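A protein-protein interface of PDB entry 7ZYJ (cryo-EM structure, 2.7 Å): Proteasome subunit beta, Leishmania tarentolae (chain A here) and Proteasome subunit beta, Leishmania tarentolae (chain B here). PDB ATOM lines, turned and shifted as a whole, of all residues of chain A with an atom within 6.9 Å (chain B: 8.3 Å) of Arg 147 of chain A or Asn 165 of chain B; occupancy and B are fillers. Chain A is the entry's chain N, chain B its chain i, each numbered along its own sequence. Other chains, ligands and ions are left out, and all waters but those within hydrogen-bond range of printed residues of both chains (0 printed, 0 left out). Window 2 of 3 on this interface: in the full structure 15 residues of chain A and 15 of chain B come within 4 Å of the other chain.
Of the 20 printed residues of chain B, 4 touch a printed residue of chain A. Printed residues of chain B that touch a printed residue of chain A: Ile 132, Ala 133, Lys 161 and Asn 165. Hydrophobic or aromatic side chains of chain B that line the printed part of chain A: Ile 132 and Ala 133. Hydrophobic or aromatic side chains of chain A within 4 Å of the printed part of chain B: Tyr 140 and Pro 144. Among the printed residues, 6 pairs touch across the chains.
Cys 132 of chain A touches none of the printed residues of chain B. Of the printed residues of chain B, Pro 144 of chain A touches Ala 133 (3.8 Å) and Asn 165 (3.4 Å). Of chain B, only Asn 165 (3.4 Å) comes within 4 Å of Arg 147 of chain A. Printed residues of chain B within 4 Å of Gln 148 of chain A: Lys 161 (3.5 Å). Printed residues of chain A within 4 Å of Ala 133 of chain B: Tyr 140 and Pro 144. Of the printed residues of chain A, Lys 161 of chain B touches Gln 148 (3.5 Å). Asn 165 of chain B touches just these residues of chain A: Pro 144 (3.4 Å) and Arg 147 (3.4 Å).
Among the printed residues, merely in contact across the chains: Tyr 140 of chain A with Ile 132 of chain B (3.9 Å), Tyr 140 of chain A with Ala 133 of chain B (3.6 Å), Pro 144 of chain A with Ala 133 of chain B (3.8 Å) and Pro 144 of chain A with Asn 165 of chain B (3.4 Å).
NE2 of Gln 148 of chain A lies close to NZ of Lys 152 of chain A (3.1 Å). The side-chain amide nitrogen (ND2) of Asn 165 of chain B sits at hydrogen-bond distance from the backbone carbonyl oxygen (O) of Lys 161 of chain B (2.6 Å). OG of Ser 157 of chain B sits at hydrogen-bond distance from NZ of Lys 161 of chain B, at 2.9 Å.
NE2 of Gln 148 of chain A sits close to NZ of Lys 161 of chain B, 3.5 Å away. OD1 of Asn 165 of chain B lies within hydrogen-bond range of NH1 of Arg 147 of chain A (3.4 Å).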
ATOM      1  N   ILE A  10     -12.477 -21.691 -32.842  1.00  0.00           N
ATOM      2  CA  ILE A  10     -13.630 -20.948 -33.342  1.00  0.00           C
ATOM      3  C   ILE A  10     -14.134 -21.617 -34.615  1.00  0.00           C
ATOM      4  O   ILE A  10     -13.349 -22.117 -35.426  1.00  0.00           O
ATOM      5  CB  ILE A  10     -13.278 -19.461 -33.576  1.00  0.00           C
ATOM      6  CG1 ILE A  10     -14.517 -18.667 -33.995  1.00  0.00           C
ATOM      7  CG2 ILE A  10     -12.167 -19.320 -34.606  1.00  0.00           C
ATOM      8  CD1 ILE A  10     -14.479 -17.219 -33.579  1.00  0.00           C
ATOM      9  N   TRP A 128     -19.420 -29.003 -22.972  1.00  0.00           N
ATOM     10  CA  TRP A 128     -20.280 -28.021 -23.619  1.00  0.00           C
ATOM     11  C   TRP A 128     -19.871 -27.868 -25.076  1.00  0.00           C
ATOM     12  O   TRP A 128     -18.759 -28.220 -25.471  1.00  0.00           O
ATOM     13  CB  TRP A 128     -20.237 -26.662 -22.908  1.00  0.00           C
ATOM     14  CG  TRP A 128     -18.923 -25.964 -23.000  1.00  0.00           C
ATOM     15  CD1 TRP A 128     -18.607 -24.917 -23.813  1.00  0.00           C
ATOM     16  CD2 TRP A 128     -17.736 -26.274 -22.266  1.00  0.00           C
ATOM     17  NE1 TRP A 128     -17.301 -24.546 -23.622  1.00  0.00           N
ATOM     18  CE2 TRP A 128     -16.742 -25.367 -22.679  1.00  0.00           C
ATOM     19  CE3 TRP A 128     -17.419 -27.227 -21.298  1.00  0.00           C
ATOM     20  CZ2 TRP A 128     -15.455 -25.387 -22.156  1.00  0.00           C
ATOM     21  CZ3 TRP A 128     -16.148 -27.246 -20.787  1.00  0.00           C
ATOM     22  CH2 TRP A 128     -15.178 -26.332 -21.212  1.00  0.00           C
ATOM     23  N   ASP A 130     -20.214 -24.965 -28.435  1.00  0.00           N
ATOM     24  CA  ASP A 130     -20.465 -23.573 -28.783  1.00  0.00           C
ATOM     25  C   ASP A 130     -19.753 -23.278 -30.099  1.00  0.00           C
ATOM     26  O   ASP A 130     -19.114 -24.156 -30.687  1.00  0.00           O
ATOM     27  CB  ASP A 130     -20.009 -22.639 -27.657  1.00  0.00           C
ATOM     28  CG  ASP A 130     -20.740 -21.312 -27.665  1.00  0.00           C
ATOM     29  OD1 ASP A 130     -21.716 -21.172 -28.429  1.00  0.00           O
ATOM     30  OD2 ASP A 130     -20.335 -20.407 -26.906  1.00  0.00           O
ATOM     31  N   CYS A 132     -17.386 -21.009 -30.183  1.00  0.00           N
ATOM     32  CA  CYS A 132     -16.032 -20.640 -29.792  1.00  0.00           C
ATOM     33  C   CYS A 132     -15.744 -21.264 -28.436  1.00  0.00           C
ATOM     34  O   CYS A 132     -16.567 -21.171 -27.522  1.00  0.00           O
ATOM     35  CB  CYS A 132     -15.858 -19.116 -29.742  1.00  0.00           C
ATOM     36  SG  CYS A 132     -16.961 -18.257 -28.600  1.00  0.00           S
ATOM     37  N   ALA A 139      -9.612 -18.781 -21.868  1.00  0.00           N
ATOM     38  CA  ALA A 139     -11.006 -18.612 -21.478  1.00  0.00           C
ATOM     39  C   ALA A 139     -11.279 -17.204 -20.965  1.00  0.00           C
ATOM     40  O   ALA A 139     -12.368 -16.665 -21.186  1.00  0.00           O
ATOM     41  CB  ALA A 139     -11.386 -19.647 -20.420  1.00  0.00           C
ATOM     42  N   TYR A 140     -10.313 -16.599 -20.277  1.00  0.00           N
ATOM     43  CA  TYR A 140     -10.479 -15.247 -19.758  1.00  0.00           C
ATOM     44  C   TYR A 140      -9.965 -14.182 -20.713  1.00  0.00           C
ATOM     45  O   TYR A 140     -10.454 -13.048 -20.684  1.00  0.00           O
ATOM     46  CB  TYR A 140      -9.761 -15.105 -18.413  1.00  0.00           C
ATOM     47  CG  TYR A 140      -9.978 -16.268 -17.473  1.00  0.00           C
ATOM     48  CD1 TYR A 140     -11.107 -16.335 -16.670  1.00  0.00           C
ATOM     49  CD2 TYR A 140      -9.049 -17.297 -17.387  1.00  0.00           C
ATOM     50  CE1 TYR A 140     -11.308 -17.396 -15.810  1.00  0.00           C
ATOM     51  CE2 TYR A 140      -9.243 -18.363 -16.530  1.00  0.00           C
ATOM     52  CZ  TYR A 140     -10.374 -18.406 -15.743  1.00  0.00           C
ATOM     53  OH  TYR A 140     -10.572 -19.464 -14.887  1.00  0.00           O
ATOM     54  N   ALA A 142      -8.813 -14.742 -24.489  1.00  0.00           N
ATOM     55  CA  ALA A 142      -9.191 -14.846 -25.895  1.00  0.00           C
ATOM     56  C   ALA A 142     -10.700 -14.940 -26.083  1.00  0.00           C
ATOM     57  O   ALA A 142     -11.239 -14.397 -27.054  1.00  0.00           O
ATOM     58  CB  ALA A 142      -8.505 -16.054 -26.529  1.00  0.00           C
ATOM     59  N   LEU A 143     -11.391 -15.627 -25.175  1.00  0.00           N
ATOM     60  CA  LEU A 143     -12.805 -15.923 -25.387  1.00  0.00           C
ATOM     61  C   LEU A 143     -13.684 -14.684 -25.535  1.00  0.00           C
ATOM     62  O   LEU A 143     -14.567 -14.697 -26.410  1.00  0.00           O
ATOM     63  CB  LEU A 143     -13.311 -16.828 -24.255  1.00  0.00           C
ATOM     64  CG  LEU A 143     -14.561 -17.663 -24.531  1.00  0.00           C
ATOM     65  CD1 LEU A 143     -14.372 -18.511 -25.774  1.00  0.00           C
ATOM     66  CD2 LEU A 143     -14.865 -18.540 -23.333  1.00  0.00           C
ATOM     67  N   PRO A 144     -13.540 -13.620 -24.731  1.00  0.00           N
ATOM     68  CA  PRO A 144     -14.348 -12.415 -24.993  1.00  0.00           C
ATOM     69  C   PRO A 144     -14.151 -11.840 -26.385  1.00  0.00           C
ATOM     70  O   PRO A 144     -15.127 -11.429 -27.028  1.00  0.00           O
ATOM     71  CB  PRO A 144     -13.876 -11.443 -23.906  1.00  0.00           C
ATOM     72  CG  PRO A 144     -13.447 -12.320 -22.797  1.00  0.00           C
ATOM     73  CD  PRO A 144     -12.815 -13.512 -23.451  1.00  0.00           C
ATOM     74  N   LEU A 145     -12.910 -11.815 -26.878  1.00  0.00           N
ATOM     75  CA  LEU A 145     -12.657 -11.298 -28.218  1.00  0.00           C
ATOM     76  C   LEU A 145     -13.295 -12.183 -29.279  1.00  0.00           C
ATOM     77  O   LEU A 145     -13.859 -11.683 -30.259  1.00  0.00           O
ATOM     78  CB  LEU A 145     -11.152 -11.173 -28.456  1.00  0.00           C
ATOM     79  CG  LEU A 145     -10.383 -10.289 -27.473  1.00  0.00           C
ATOM     80  CD1 LEU A 145      -8.897 -10.323 -27.777  1.00  0.00           C
ATOM     81  CD2 LEU A 145     -10.911  -8.866 -27.511  1.00  0.00           C
ATOM     82  N   LEU A 146     -13.214 -13.504 -29.102  1.00  0.00           N
ATOM     83  CA  LEU A 146     -13.843 -14.420 -30.046  1.00  0.00           C
ATOM     84  C   LEU A 146     -15.354 -14.242 -30.062  1.00  0.00           C
ATOM     85  O   LEU A 146     -15.975 -14.238 -31.130  1.00  0.00           O
ATOM     86  CB  LEU A 146     -13.477 -15.861 -29.697  1.00  0.00           C
ATOM     87  CG  LEU A 146     -12.008 -16.254 -29.868  1.00  0.00           C
ATOM     88  CD1 LEU A 146     -11.759 -17.641 -29.304  1.00  0.00           C
ATOM     89  CD2 LEU A 146     -11.605 -16.188 -31.331  1.00  0.00           C
ATOM     90  N   ARG A 147     -15.966 -14.093 -28.884  1.00  0.00           N
ATOM     91  CA  ARG A 147     -17.408 -13.884 -28.823  1.00  0.00           C
ATOM     92  C   ARG A 147     -17.807 -12.570 -29.481  1.00  0.00           C
ATOM     93  O   ARG A 147     -18.812 -12.508 -30.199  1.00  0.00           O
ATOM     94  CB  ARG A 147     -17.887 -13.925 -27.374  1.00  0.00           C
ATOM     95  CG  ARG A 147     -18.133 -15.323 -26.853  1.00  0.00           C
ATOM     96  CD  ARG A 147     -18.043 -15.384 -25.343  1.00  0.00           C
ATOM     97  NE  ARG A 147     -18.293 -16.733 -24.853  1.00  0.00           N
ATOM     98  CZ  ARG A 147     -18.026 -17.147 -23.623  1.00  0.00           C
ATOM     99  NH1 ARG A 147     -17.502 -16.336 -22.719  1.00  0.00           N
ATOM    100  NH2 ARG A 147     -18.287 -18.407 -23.293  1.00  0.00           N
ATOM    101  N   GLN A 148     -17.034 -11.507 -29.247  1.00  0.00           N
ATOM    102  CA  GLN A 148     -17.329 -10.236 -29.896  1.00  0.00           C
ATOM    103  C   GLN A 148     -17.206 -10.340 -31.410  1.00  0.00           C
ATOM    104  O   GLN A 148     -18.067  -9.834 -32.138  1.00  0.00           O
ATOM    105  CB  GLN A 148     -16.405  -9.145 -29.356  1.00  0.00           C
ATOM    106  CG  GLN A 148     -16.559  -7.803 -30.047  1.00  0.00           C
ATOM    107  CD  GLN A 148     -15.285  -6.988 -30.023  1.00  0.00           C
ATOM    108  OE1 GLN A 148     -14.192  -7.529 -29.858  1.00  0.00           O
ATOM    109  NE2 GLN A 148     -15.419  -5.678 -30.183  1.00  0.00           N
ATOM    110  N   ALA A 149     -16.160 -11.010 -31.901  1.00  0.00           N
ATOM    111  CA  ALA A 149     -16.003 -11.194 -33.339  1.00  0.00           C
ATOM    112  C   ALA A 149     -17.145 -12.011 -33.926  1.00  0.00           C
ATOM    113  O   ALA A 149     -17.606 -11.722 -35.036  1.00  0.00           O
ATOM    114  CB  ALA A 149     -14.664 -11.863 -33.641  1.00  0.00           C
ATOM    115  N   LEU A 150     -17.604 -13.036 -33.205  1.00  0.00           N
ATOM    116  CA  LEU A 150     -18.741 -13.822 -33.671  1.00  0.00           C
ATOM    117  C   LEU A 150     -20.012 -12.984 -33.726  1.00  0.00           C
ATOM    118  O   LEU A 150     -20.794 -13.097 -34.677  1.00  0.00           O
ATOM    119  CB  LEU A 150     -18.942 -15.037 -32.768  1.00  0.00           C
ATOM    120  CG  LEU A 150     -18.098 -16.272 -33.080  1.00  0.00           C
ATOM    121  CD1 LEU A 150     -18.166 -17.257 -31.929  1.00  0.00           C
ATOM    122  CD2 LEU A 150     -18.553 -16.922 -34.373  1.00  0.00           C
ATOM    123  N   GLU A 151     -20.241 -12.143 -32.717  1.00  0.00           N
ATOM    124  CA  GLU A 151     -21.486 -11.387 -32.657  1.00  0.00           C
ATOM    125  C   GLU A 151     -21.489 -10.146 -33.541  1.00  0.00           C
ATOM    126  O   GLU A 151     -22.569  -9.610 -33.811  1.00  0.00           O
ATOM    127  CB  GLU A 151     -21.798 -10.990 -31.211  1.00  0.00           C
ATOM    128  CG  GLU A 151     -20.918  -9.892 -30.650  1.00  0.00           C
ATOM    129  CD  GLU A 151     -21.214  -9.605 -29.191  1.00  0.00           C
ATOM    130  OE1 GLU A 151     -22.389  -9.344 -28.863  1.00  0.00           O
ATOM    131  OE2 GLU A 151     -20.271  -9.645 -28.372  1.00  0.00           O
ATOM    132  N   LYS A 152     -20.329  -9.673 -34.004  1.00  0.00           N
ATOM    133  CA  LYS A 152     -20.338  -8.583 -34.976  1.00  0.00           C
ATOM    134  C   LYS A 152     -20.797  -9.023 -36.358  1.00  0.00           C
ATOM    135  O   LYS A 152     -21.061  -8.163 -37.205  1.00  0.00           O
ATOM    136  CB  LYS A 152     -18.956  -7.933 -35.086  1.00  0.00           C
ATOM    137  CG  LYS A 152     -18.459  -7.297 -33.804  1.00  0.00           C
ATOM    138  CD  LYS A 152     -19.284  -6.070 -33.453  1.00  0.00           C
ATOM    139  CE  LYS A 152     -18.798  -5.428 -32.167  1.00  0.00           C
ATOM    140  NZ  LYS A 152     -17.446  -4.827 -32.335  1.00  0.00           N
ATOM    141  N   ILE A 165      -8.845 -13.033 -36.399  1.00  0.00           N
ATOM    142  CA  ILE A 165      -9.177 -12.857 -34.990  1.00  0.00           C
ATOM    143  C   ILE A 165      -8.476 -13.905 -34.136  1.00  0.00           C
ATOM    144  O   ILE A 165      -8.109 -13.634 -32.985  1.00  0.00           O
ATOM    145  CB  ILE A 165     -10.706 -12.867 -34.786  1.00  0.00           C
ATOM    146  CG1 ILE A 165     -11.056 -12.520 -33.337  1.00  0.00           C
ATOM    147  CG2 ILE A 165     -11.305 -14.205 -35.172  1.00  0.00           C
ATOM    148  CD1 ILE A 165     -10.685 -11.110 -32.940  1.00  0.00           C
ATOM    149  N   THR B   2     -15.140  -3.606 -13.114  1.00  0.00           N
ATOM    150  CA  THR B   2     -14.200  -3.414 -14.216  1.00  0.00           C
ATOM    151  C   THR B   2     -13.953  -1.922 -14.370  1.00  0.00           C
ATOM    152  O   THR B   2     -14.884  -1.171 -14.676  1.00  0.00           O
ATOM    153  CB  THR B   2     -14.736  -4.012 -15.518  1.00  0.00           C
ATOM    154  OG1 THR B   2     -15.203  -5.345 -15.279  1.00  0.00           O
ATOM    155  CG2 THR B   2     -13.647  -4.043 -16.576  1.00  0.00           C
ATOM    156  N   SER B 129     -12.239  -7.250 -11.037  1.00  0.00           N
ATOM    157  CA  SER B 129     -12.425  -8.671 -11.313  1.00  0.00           C
ATOM    158  C   SER B 129     -12.542  -8.946 -12.807  1.00  0.00           C
ATOM    159  O   SER B 129     -12.105 -10.002 -13.277  1.00  0.00           O
ATOM    160  CB  SER B 129     -13.658  -9.189 -10.575  1.00  0.00           C
ATOM    161  OG  SER B 129     -14.811  -8.444 -10.925  1.00  0.00           O
ATOM    162  N   GLY B 130     -13.125  -8.020 -13.563  1.00  0.00           N
ATOM    163  CA  GLY B 130     -13.259  -8.186 -14.996  1.00  0.00           C
ATOM    164  C   GLY B 130     -12.163  -7.489 -15.774  1.00  0.00           C
ATOM    165  O   GLY B 130     -12.316  -7.216 -16.967  1.00  0.00           O
ATOM    166  N   ILE B 132      -9.101  -8.565 -16.687  1.00  0.00           N
ATOM    167  CA  ILE B 132      -8.398  -9.353 -17.695  1.00  0.00           C
ATOM    168  C   ILE B 132      -9.146  -9.323 -19.020  1.00  0.00           C
ATOM    169  O   ILE B 132      -8.572  -8.991 -20.063  1.00  0.00           O
ATOM    170  CB  ILE B 132      -8.188 -10.791 -17.190  1.00  0.00           C
ATOM    171  CG1 ILE B 132      -7.187 -10.803 -16.033  1.00  0.00           C
ATOM    172  CG2 ILE B 132      -7.718 -11.691 -18.317  1.00  0.00           C
ATOM    173  CD1 ILE B 132      -6.873 -12.184 -15.509  1.00  0.00           C
ATOM    174  N   ALA B 133     -10.447  -9.621 -18.994  1.00  0.00           N
ATOM    175  CA  ALA B 133     -11.245  -9.543 -20.211  1.00  0.00           C
ATOM    176  C   ALA B 133     -11.243  -8.135 -20.788  1.00  0.00           C
ATOM    177  O   ALA B 133     -11.321  -7.967 -22.009  1.00  0.00           O
ATOM    178  CB  ALA B 133     -12.674 -10.005 -19.937  1.00  0.00           C
ATOM    179  N   ALA B 134     -11.158  -7.117 -19.930  1.00  0.00           N
ATOM    180  CA  ALA B 134     -11.002  -5.755 -20.426  1.00  0.00           C
ATOM    181  C   ALA B 134      -9.637  -5.567 -21.073  1.00  0.00           C
ATOM    182  O   ALA B 134      -9.529  -5.002 -22.167  1.00  0.00           O
ATOM    183  CB  ALA B 134     -11.207  -4.757 -19.288  1.00  0.00           C
ATOM    184  N   SER B 157     -15.849  -0.302 -25.110  1.00  0.00           N
ATOM    185  CA  SER B 157     -15.770  -1.695 -25.537  1.00  0.00           C
ATOM    186  C   SER B 157     -15.047  -2.553 -24.505  1.00  0.00           C
ATOM    187  O   SER B 157     -15.481  -3.673 -24.206  1.00  0.00           O
ATOM    188  CB  SER B 157     -15.079  -1.784 -26.896  1.00  0.00           C
ATOM    189  OG  SER B 157     -14.596  -3.091 -27.138  1.00  0.00           O
ATOM    190  N   ALA B 158     -13.946  -2.044 -23.946  1.00  0.00           N
ATOM    191  CA  ALA B 158     -13.227  -2.793 -22.921  1.00  0.00           C
ATOM    192  C   ALA B 158     -14.077  -2.984 -21.673  1.00  0.00           C
ATOM    193  O   ALA B 158     -13.994  -4.031 -21.022  1.00  0.00           O
ATOM    194  CB  ALA B 158     -11.919  -2.086 -22.570  1.00  0.00           C
ATOM    195  N   ILE B 159     -14.888  -1.986 -21.318  1.00  0.00           N
ATOM    196  CA  ILE B 159     -15.788  -2.136 -20.181  1.00  0.00           C
ATOM    197  C   ILE B 159     -16.865  -3.169 -20.490  1.00  0.00           C
ATOM    198  O   ILE B 159     -17.222  -3.985 -19.636  1.00  0.00           O
ATOM    199  CB  ILE B 159     -16.395  -0.777 -19.792  1.00  0.00           C
ATOM    200  CG1 ILE B 159     -15.323   0.129 -19.184  1.00  0.00           C
ATOM    201  CG2 ILE B 159     -17.537  -0.959 -18.807  1.00  0.00           C
ATOM    202  CD1 ILE B 159     -14.840  -0.326 -17.831  1.00  0.00           C
ATOM    203  N   ARG B 160     -17.395  -3.152 -21.717  1.00  0.00           N
ATOM    204  CA  ARG B 160     -18.407  -4.131 -22.101  1.00  0.00           C
ATOM    205  C   ARG B 160     -17.852  -5.548 -22.086  1.00  0.00           C
ATOM    206  O   ARG B 160     -18.594  -6.501 -21.825  1.00  0.00           O
ATOM    207  CB  ARG B 160     -18.966  -3.802 -23.484  1.00  0.00           C
ATOM    208  CG  ARG B 160     -19.899  -2.609 -23.512  1.00  0.00           C
ATOM    209  CD  ARG B 160     -20.542  -2.454 -24.878  1.00  0.00           C
ATOM    210  NE  ARG B 160     -19.556  -2.415 -25.950  1.00  0.00           N
ATOM    211  CZ  ARG B 160     -19.258  -1.334 -26.656  1.00  0.00           C
ATOM    212  NH1 ARG B 160     -19.846  -0.172 -26.423  1.00  0.00           N
ATOM    213  NH2 ARG B 160     -18.350  -1.420 -27.623  1.00  0.00           N
ATOM    214  N   LYS B 161     -16.558  -5.710 -22.377  1.00  0.00           N
ATOM    215  CA  LYS B 161     -15.955  -7.037 -22.290  1.00  0.00           C
ATOM    216  C   LYS B 161     -16.023  -7.593 -20.875  1.00  0.00           C
ATOM    217  O   LYS B 161     -16.273  -8.788 -20.690  1.00  0.00           O
ATOM    218  CB  LYS B 161     -14.504  -7.006 -22.773  1.00  0.00           C
ATOM    219  CG  LYS B 161     -14.338  -6.540 -24.201  1.00  0.00           C
ATOM    220  CD  LYS B 161     -15.123  -7.422 -25.151  1.00  0.00           C
ATOM    221  CE  LYS B 161     -15.064  -6.891 -26.568  1.00  0.00           C
ATOM    222  NZ  LYS B 161     -15.834  -5.628 -26.713  1.00  0.00           N
ATOM    223  N   GLY B 162     -15.798  -6.753 -19.870  1.00  0.00           N
ATOM    224  CA  GLY B 162     -15.945  -7.180 -18.492  1.00  0.00           C
ATOM    225  C   GLY B 162     -17.395  -7.277 -18.069  1.00  0.00           C
ATOM    226  O   GLY B 162     -17.738  -8.039 -17.164  1.00  0.00           O
ATOM    227  N   ILE B 163     -18.260  -6.500 -18.720  1.00  0.00           N
ATOM    228  CA  ILE B 163     -19.680  -6.509 -18.376  1.00  0.00           C
ATOM    229  C   ILE B 163     -20.291  -7.871 -18.680  1.00  0.00           C
ATOM    230  O   ILE B 163     -21.045  -8.429 -17.875  1.00  0.00           O
ATOM    231  CB  ILE B 163     -20.416  -5.380 -19.120  1.00  0.00           C
ATOM    232  CG1 ILE B 163     -20.218  -4.047 -18.399  1.00  0.00           C
ATOM    233  CG2 ILE B 163     -21.897  -5.697 -19.261  1.00  0.00           C
ATOM    234  CD1 ILE B 163     -20.820  -2.875 -19.128  1.00  0.00           C
ATOM    235  N   PHE B 164     -19.963  -8.431 -19.843  1.00  0.00           N
ATOM    236  CA  PHE B 164     -20.614  -9.646 -20.312  1.00  0.00           C
ATOM    237  C   PHE B 164     -19.878 -10.917 -19.911  1.00  0.00           C
ATOM    238  O   PHE B 164     -20.486 -11.992 -19.893  1.00  0.00           O
ATOM    239  CB  PHE B 164     -20.761  -9.602 -21.833  1.00  0.00           C
ATOM    240  CG  PHE B 164     -21.809  -8.641 -22.307  1.00  0.00           C
ATOM    241  CD1 PHE B 164     -23.097  -8.696 -21.803  1.00  0.00           C
ATOM    242  CD2 PHE B 164     -21.506  -7.675 -23.250  1.00  0.00           C
ATOM    243  CE1 PHE B 164     -24.064  -7.809 -22.234  1.00  0.00           C
ATOM    244  CE2 PHE B 164     -22.467  -6.786 -23.686  1.00  0.00           C
ATOM    245  CZ  PHE B 164     -23.748  -6.853 -23.177  1.00  0.00           C
ATOM    246  N   ASN B 165     -18.589 -10.826 -19.594  1.00  0.00           N
ATOM    247  CA  ASN B 165     -17.799 -11.994 -19.234  1.00  0.00           C
ATOM    248  C   ASN B 165     -17.466 -12.061 -17.751  1.00  0.00           C
ATOM    249  O   ASN B 165     -16.794 -13.005 -17.324  1.00  0.00           O
ATOM    250  CB  ASN B 165     -16.509 -12.026 -20.063  1.00  0.00           C
ATOM    251  CG  ASN B 165     -16.779 -12.017 -21.555  1.00  0.00           C
ATOM    252  OD1 ASN B 165     -17.061 -13.056 -22.151  1.00  0.00           O
ATOM    253  ND2 ASN B 165     -16.704 -10.841 -22.164  1.00  0.00           N
ATOM    254  N   ASP B 166     -17.919 -11.095 -16.954  1.00  0.00           N
ATOM    255  CA  ASP B 166     -17.730 -11.115 -15.512  1.00  0.00           C
ATOM    256  C   ASP B 166     -19.102 -10.983 -14.862  1.00  0.00           C
ATOM    257  O   ASP B 166     -19.834 -10.021 -15.152  1.00  0.00           O
ATOM    258  CB  ASP B 166     -16.798  -9.978 -15.060  1.00  0.00           C
ATOM    259  CG  ASP B 166     -16.400 -10.075 -13.596  1.00  0.00           C
ATOM    260  OD1 ASP B 166     -16.851 -10.999 -12.892  1.00  0.00           O
ATOM    261  OD2 ASP B 166     -15.639  -9.200 -13.138  1.00  0.00           O
ATOM    262  N   PRO B 167     -19.496 -11.922 -13.997  1.00  0.00           N
ATOM    263  CA  PRO B 167     -20.788 -11.784 -13.305  1.00  0.00           C
ATOM    264  C   PRO B 167     -20.853 -10.605 -12.347  1.00  0.00           C
ATOM    265  O   PRO B 167     -21.961 -10.206 -11.967  1.00  0.00           O
ATOM    266  CB  PRO B 167     -20.932 -13.118 -12.562  1.00  0.00           C
ATOM    267  CG  PRO B 167     -19.537 -13.638 -12.426  1.00  0.00           C
ATOM    268  CD  PRO B 167     -18.816 -13.185 -13.660  1.00  0.00           C
ATOM    269  N   TYR B 168     -19.720 -10.033 -11.948  1.00  0.00           N
ATOM    270  CA  TYR B 168     -19.695  -8.950 -10.974  1.00  0.00           C
ATOM    271  C   TYR B 168     -19.760  -7.566 -11.610  1.00  0.00           C
ATOM    272  O   TYR B 168     -19.739  -6.565 -10.887  1.00  0.00           O
ATOM    273  CB  TYR B 168     -18.439  -9.052 -10.105  1.00  0.00           C
ATOM    274  CG  TYR B 168     -18.410 -10.255  -9.190  1.00  0.00           C
ATOM    275  CD1 TYR B 168     -17.944 -11.482  -9.641  1.00  0.00           C
ATOM    276  CD2 TYR B 168     -18.840 -10.162  -7.873  1.00  0.00           C
ATOM    277  CE1 TYR B 168     -17.913 -12.584  -8.808  1.00  0.00           C
ATOM    278  CE2 TYR B 168     -18.812 -11.258  -7.033  1.00  0.00           C
ATOM    279  CZ  TYR B 168     -18.348 -12.467  -7.506  1.00  0.00           C
ATOM    280  OH  TYR B 168     -18.316 -13.561  -6.674  1.00  0.00           O
ATOM    281  N   SER B 169     -19.838  -7.482 -12.937  1.00  0.00           N
ATOM    282  CA  SER B 169     -19.855  -6.205 -13.637  1.00  0.00           C
ATOM    283  C   SER B 169     -21.066  -6.133 -14.553  1.00  0.00           C
ATOM    284  O   SER B 169     -21.554  -7.156 -15.040  1.00  0.00           O
ATOM    285  CB  SER B 169     -18.576  -6.003 -14.460  1.00  0.00           C
ATOM    286  OG  SER B 169     -17.427  -6.017 -13.636  1.00  0.00           O
ATOM    287  N   GLY B 170     -21.552  -4.922 -14.782  1.00  0.00           N
ATOM    288  CA  GLY B 170     -22.559  -4.721 -15.802  1.00  0.00           C
ATOM    289  C   GLY B 170     -23.436  -3.515 -15.526  1.00  0.00           C
ATOM    290  O   GLY B 170     -23.131  -2.666 -14.689  1.00  0.00           O
